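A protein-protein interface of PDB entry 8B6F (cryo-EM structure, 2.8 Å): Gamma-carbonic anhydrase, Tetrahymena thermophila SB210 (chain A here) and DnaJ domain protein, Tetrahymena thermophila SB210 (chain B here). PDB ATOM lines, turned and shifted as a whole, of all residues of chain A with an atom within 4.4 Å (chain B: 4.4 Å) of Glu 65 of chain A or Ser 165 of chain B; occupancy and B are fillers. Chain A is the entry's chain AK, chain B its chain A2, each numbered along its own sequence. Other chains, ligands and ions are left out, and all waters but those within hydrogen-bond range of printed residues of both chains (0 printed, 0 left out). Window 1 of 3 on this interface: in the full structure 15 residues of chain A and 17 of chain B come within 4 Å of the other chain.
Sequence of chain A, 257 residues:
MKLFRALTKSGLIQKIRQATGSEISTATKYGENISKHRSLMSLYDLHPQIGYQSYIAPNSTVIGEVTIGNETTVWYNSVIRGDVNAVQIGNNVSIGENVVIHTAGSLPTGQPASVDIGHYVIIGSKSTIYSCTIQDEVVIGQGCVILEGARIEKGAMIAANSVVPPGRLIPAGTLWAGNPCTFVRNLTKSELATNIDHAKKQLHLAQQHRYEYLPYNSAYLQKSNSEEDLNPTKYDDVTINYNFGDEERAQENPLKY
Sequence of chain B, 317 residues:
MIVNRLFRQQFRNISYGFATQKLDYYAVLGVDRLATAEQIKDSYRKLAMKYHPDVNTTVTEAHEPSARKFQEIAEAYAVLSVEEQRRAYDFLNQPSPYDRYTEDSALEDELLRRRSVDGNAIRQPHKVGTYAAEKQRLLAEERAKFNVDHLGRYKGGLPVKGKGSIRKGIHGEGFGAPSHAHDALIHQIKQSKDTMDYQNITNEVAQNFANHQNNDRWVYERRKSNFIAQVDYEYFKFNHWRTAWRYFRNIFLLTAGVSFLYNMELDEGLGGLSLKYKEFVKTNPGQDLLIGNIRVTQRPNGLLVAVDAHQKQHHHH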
ATOM      1  N   LEU A  46      29.638  29.027 -17.237  1.00  0.00           N
ATOM      2  CA  LEU A  46      28.215  29.336 -17.343  1.00  0.00           C
ATOM      3  C   LEU A  46      28.010  30.769 -16.877  1.00  0.00           C
ATOM      4  O   LEU A  46      27.782  31.026 -15.693  1.00  0.00           O
ATOM      5  CB  LEU A  46      27.389  28.348 -16.523  1.00  0.00           C
ATOM      6  CG  LEU A  46      27.723  26.867 -16.726  1.00  0.00           C
ATOM      7  CD1 LEU A  46      26.848  26.005 -15.840  1.00  0.00           C
ATOM      8  CD2 LEU A  46      27.572  26.455 -18.179  1.00  0.00           C
ATOM      9  N   ILE A  63      22.623  32.498 -10.861  1.00  0.00           N
ATOM     10  CA  ILE A  63      23.875  31.768 -10.999  1.00  0.00           C
ATOM     11  C   ILE A  63      23.713  30.705 -12.074  1.00  0.00           C
ATOM     12  O   ILE A  63      22.681  30.030 -12.142  1.00  0.00           O
ATOM     13  CB  ILE A  63      24.309  31.135  -9.662  1.00  0.00           C
ATOM     14  CG1 ILE A  63      25.646  30.413  -9.831  1.00  0.00           C
ATOM     15  CG2 ILE A  63      23.238  30.183  -9.147  1.00  0.00           C
ATOM     16  CD1 ILE A  63      26.274  29.980  -8.530  1.00  0.00           C
ATOM     17  N   GLY A  64      24.732  30.562 -12.910  1.00  0.00           N
ATOM     18  CA  GLY A  64      24.755  29.530 -13.922  1.00  0.00           C
ATOM     19  C   GLY A  64      24.435  30.051 -15.307  1.00  0.00           C
ATOM     20  O   GLY A  64      24.559  31.238 -15.615  1.00  0.00           O
ATOM     21  N   GLU A  65      24.011  29.121 -16.163  1.00  0.00           N
ATOM     22  CA  GLU A  65      23.683  29.427 -17.555  1.00  0.00           C
ATOM     23  C   GLU A  65      22.252  29.953 -17.607  1.00  0.00           C
ATOM     24  O   GLU A  65      21.296  29.239 -17.923  1.00  0.00           O
ATOM     25  CB  GLU A  65      23.867  28.193 -18.429  1.00  0.00           C
ATOM     26  CG  GLU A  65      23.850  28.488 -19.914  1.00  0.00           C
ATOM     27  CD  GLU A  65      24.111  27.254 -20.752  1.00  0.00           C
ATOM     28  OE1 GLU A  65      23.997  26.132 -20.214  1.00  0.00           O
ATOM     29  OE2 GLU A  65      24.435  27.404 -21.949  1.00  0.00           O
ATOM     30  N   VAL A  66      22.108  31.235 -17.284  1.00  0.00           N
ATOM     31  CA  VAL A  66      20.817  31.913 -17.260  1.00  0.00           C
ATOM     32  C   VAL A  66      20.878  33.087 -18.224  1.00  0.00           C
ATOM     33  O   VAL A  66      21.790  33.917 -18.141  1.00  0.00           O
ATOM     34  CB  VAL A  66      20.451  32.388 -15.842  1.00  0.00           C
ATOM     35  CG1 VAL A  66      19.126  33.141 -15.849  1.00  0.00           C
ATOM     36  CG2 VAL A  66      20.387  31.212 -14.888  1.00  0.00           C
ATOM     37  N   THR A  67      19.911  33.157 -19.132  1.00  0.00           N
ATOM     38  CA  THR A  67      19.805  34.250 -20.088  1.00  0.00           C
ATOM     39  C   THR A  67      18.538  35.040 -19.797  1.00  0.00           C
ATOM     40  O   THR A  67      17.446  34.467 -19.728  1.00  0.00           O
ATOM     41  CB  THR A  67      19.779  33.725 -21.525  1.00  0.00           C
ATOM     42  OG1 THR A  67      20.928  32.902 -21.756  1.00  0.00           O
ATOM     43  CG2 THR A  67      19.783  34.878 -22.517  1.00  0.00           C
ATOM     44  N   GLY A  82      20.800  28.101 -13.227  1.00  0.00           N
ATOM     45  CA  GLY A  82      20.905  27.398 -14.491  1.00  0.00           C
ATOM     46  C   GLY A  82      22.117  26.491 -14.511  1.00  0.00           C
ATOM     47  O   GLY A  82      22.721  26.254 -15.560  1.00  0.00           O
ATOM     48  N   ASN A  85      21.198  22.950 -16.018  1.00  0.00           N
ATOM     49  CA  ASN A  85      20.758  23.070 -17.402  1.00  0.00           C
ATOM     50  C   ASN A  85      20.517  24.545 -17.688  1.00  0.00           C
ATOM     51  O   ASN A  85      20.486  25.376 -16.778  1.00  0.00           O
ATOM     52  CB  ASN A  85      19.498  22.240 -17.659  1.00  0.00           C
ATOM     53  CG  ASN A  85      19.654  21.299 -18.834  1.00  0.00           C
ATOM     54  OD1 ASN A  85      20.091  21.700 -19.912  1.00  0.00           O
ATOM     55  ND2 ASN A  85      19.308  20.034 -18.628  1.00  0.00           N
ATOM     56  N   ALA A  86      20.346  24.860 -18.969  1.00  0.00           N
ATOM     57  CA  ALA A  86      20.164  26.242 -19.382  1.00  0.00           C
ATOM     58  C   ALA A  86      18.806  26.773 -18.939  1.00  0.00           C
ATOM     59  O   ALA A  86      17.844  26.022 -18.767  1.00  0.00           O
ATOM     60  CB  ALA A  86      20.303  26.364 -20.899  1.00  0.00           C
ATOM     61  N   VAL A  87      18.739  28.088 -18.744  1.00  0.00           N
ATOM     62  CA  VAL A  87      17.506  28.783 -18.396  1.00  0.00           C
ATOM     63  C   VAL A  87      17.354  29.974 -19.329  1.00  0.00           C
ATOM     64  O   VAL A  87      18.261  30.807 -19.430  1.00  0.00           O
ATOM     65  CB  VAL A  87      17.500  29.244 -16.925  1.00  0.00           C
ATOM     66  CG1 VAL A  87      16.226  30.011 -16.604  1.00  0.00           C
ATOM     67  CG2 VAL A  87      17.652  28.055 -15.996  1.00  0.00           C
ATOM     68  N   LYS B 163      35.121  22.610 -19.967  1.00  0.00           N
ATOM     69  CA  LYS B 163      34.479  21.901 -21.071  1.00  0.00           C
ATOM     70  C   LYS B 163      33.184  22.572 -21.517  1.00  0.00           C
ATOM     71  O   LYS B 163      32.319  21.913 -22.099  1.00  0.00           O
ATOM     72  CB  LYS B 163      34.222  20.441 -20.694  1.00  0.00           C
ATOM     73  CG  LYS B 163      35.490  19.605 -20.626  1.00  0.00           C
ATOM     74  CD  LYS B 163      35.181  18.126 -20.474  1.00  0.00           C
ATOM     75  CE  LYS B 163      36.434  17.282 -20.617  1.00  0.00           C
ATOM     76  NZ  LYS B 163      37.494  17.693 -19.658  1.00  0.00           N
ATOM     77  N   GLY B 164      33.035  23.866 -21.258  1.00  0.00           N
ATOM     78  CA  GLY B 164      31.878  24.585 -21.769  1.00  0.00           C
ATOM     79  C   GLY B 164      30.575  24.008 -21.256  1.00  0.00           C
ATOM     80  O   GLY B 164      30.406  23.755 -20.059  1.00  0.00           O
ATOM     81  N   SER B 165      29.629  23.804 -22.172  1.00  0.00           N
ATOM     82  CA  SER B 165      28.300  23.322 -21.815  1.00  0.00           C
ATOM     83  C   SER B 165      28.267  21.836 -21.487  1.00  0.00           C
ATOM     84  O   SER B 165      27.239  21.352 -21.006  1.00  0.00           O
ATOM     85  CB  SER B 165      27.316  23.607 -22.952  1.00  0.00           C
ATOM     86  OG  SER B 165      27.192  25.000 -23.179  1.00  0.00           O
ATOM     87  N   ILE B 166      29.349  21.100 -21.746  1.00  0.00           N
ATOM     88  CA  ILE B 166      29.375  19.686 -21.404  1.00  0.00           C
ATOM     89  C   ILE B 166      29.204  19.532 -19.901  1.00  0.00           C
ATOM     90  O   ILE B 166      29.809  20.265 -19.108  1.00  0.00           O
ATOM     91  CB  ILE B 166      30.683  19.037 -21.885  1.00  0.00           C
ATOM     92  CG1 ILE B 166      30.831  19.211 -23.400  1.00  0.00           C
ATOM     93  CG2 ILE B 166      30.710  17.559 -21.505  1.00  0.00           C
ATOM     94  CD1 ILE B 166      32.135  18.692 -23.962  1.00  0.00           C
ATOM     95  N   ARG B 167      28.373  18.573 -19.500  1.00  0.00           N
ATOM     96  CA  ARG B 167      28.031  18.376 -18.100  1.00  0.00           C
ATOM     97  C   ARG B 167      28.166  16.903 -17.749  1.00  0.00           C
ATOM     98  O   ARG B 167      28.037  16.028 -18.607  1.00  0.00           O
ATOM     99  CB  ARG B 167      26.613  18.876 -17.803  1.00  0.00           C
ATOM    100  CG  ARG B 167      26.294  20.172 -18.525  1.00  0.00           C
ATOM    101  CD  ARG B 167      25.387  21.082 -17.732  1.00  0.00           C
ATOM    102  NE  ARG B 167      25.123  22.311 -18.470  1.00  0.00           N
ATOM    103  CZ  ARG B 167      24.538  23.384 -17.960  1.00  0.00           C
ATOM    104  NH1 ARG B 167      24.153  23.425 -16.697  1.00  0.00           N
ATOM    105  NH2 ARG B 167      24.333  24.442 -18.737  1.00  0.00           N
ATOM    106  N   ALA B 177      27.270  18.896 -25.663  1.00  0.00           N
ATOM    107  CA  ALA B 177      26.321  19.718 -24.939  1.00  0.00           C
ATOM    108  C   ALA B 177      25.042  18.931 -24.664  1.00  0.00           C
ATOM    109  O   ALA B 177      24.760  17.935 -25.332  1.00  0.00           O
ATOM    110  CB  ALA B 177      26.012  20.986 -25.727  1.00  0.00           C
ATOM    111  N   PRO B 178      24.253  19.359 -23.672  1.00  0.00           N
ATOM    112  CA  PRO B 178      23.116  18.544 -23.217  1.00  0.00           C
ATOM    113  C   PRO B 178      22.204  18.027 -24.320  1.00  0.00           C
ATOM    114  O   PRO B 178      22.014  16.813 -24.434  1.00  0.00           O
ATOM    115  CB  PRO B 178      22.366  19.501 -22.283  1.00  0.00           C
ATOM    116  CG  PRO B 178      23.423  20.379 -21.741  1.00  0.00           C
ATOM    117  CD  PRO B 178      24.409  20.578 -22.857  1.00  0.00           C
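N of Gly 82 of chain A sits at hydrogen-bond distance from O of Ile 63 of chain A.
The backbone carbonyl oxygen of Glu 65 of chain A sits at hydrogen-bond distance from the backbone NH of Val 87 of chain A (2.9 Å).
The backbone carbonyl oxygen (O) of Ser 165 of chain B lies close to the guanidinium group (NE) of Arg 167 of chain B, 3.4 Å away.
The backbone NH of Glu 65 of chain A sits at hydrogen-bond distance from the backbone carbonyl oxygen of Gly 82 of chain A (3.2 Å).
Leu 46 of chain A touches Arg 167 of chain B (CD1 to NH1, 3.8 Å).
Glu 65 of chain A touches Ser 165 of chain B (OE2 to OG, 3.9 Å).
Asn 85 of chain A touches Pro 178 of chain B.
Glu 65 of chain A touches two residues of chain B.
Of chain A, only Glu 65 (3.9 Å) comes within 4 Å of Ser 165 of chain B.
Printed residues of chain B within 4 Å of Asn 85 of chain A: Arg 167 (3.1 Å) and Pro 178 (3.95 Å).
Of the printed residues of chain A, Pro 178 of chain B touches Asn 85 (3.95 Å).
Of the printed residues of chain B, Gly 82 of chain A touches Arg 167.
Of the printed residues of chain A, Arg 167 of chain B touches Leu 46 (3.8 Å), Glu 65 (2.3 Å), Gly 82 (3.4 Å) and Asn 85 (3.1 Å).
Printed residues of chain B within 4 Å of Leu 46 of chain A: Arg 167.
Ala 177 of chain B touches none of the printed residues of chain A.
Hydrophobic or aromatic side chains of chain B that line the printed part of chain A: Pro 178.
Of the 10 printed residues of chain A, 4 touch a printed residue of chain B.
Printed residues of chain A that touch a printed residue of chain B: Leu 46, Glu 65, Gly 82 and Asn 85.
Hydrophobic or aromatic side chains of chain A within 4 Å of the printed part of chain B: Leu 46.
Along chain A the printed residues that touch a printed residue of chain B span positions 46 to 85.
Among the printed residues, Asp or Glu carboxylates within 4 Å of a Lys or Arg side-chain nitrogen of the other chain: Glu 65 of chain A with Arg 167 of chain B (2.3 Å).
The side-chain carboxylate of Glu 65 of chain A lies close to the guanidinium group of Arg 167 of chain B (2.3 Å).
The guanidinium group (NH1) of Arg 167 of chain B lies close to the backbone NH (N) of Asn 85 of chain A (3.1 Å).
The backbone carbonyl oxygen of Gly 82 of chain A is in hydrogen-bond range of the guanidinium group of Arg 167 of chain B, 3.4 Å away.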
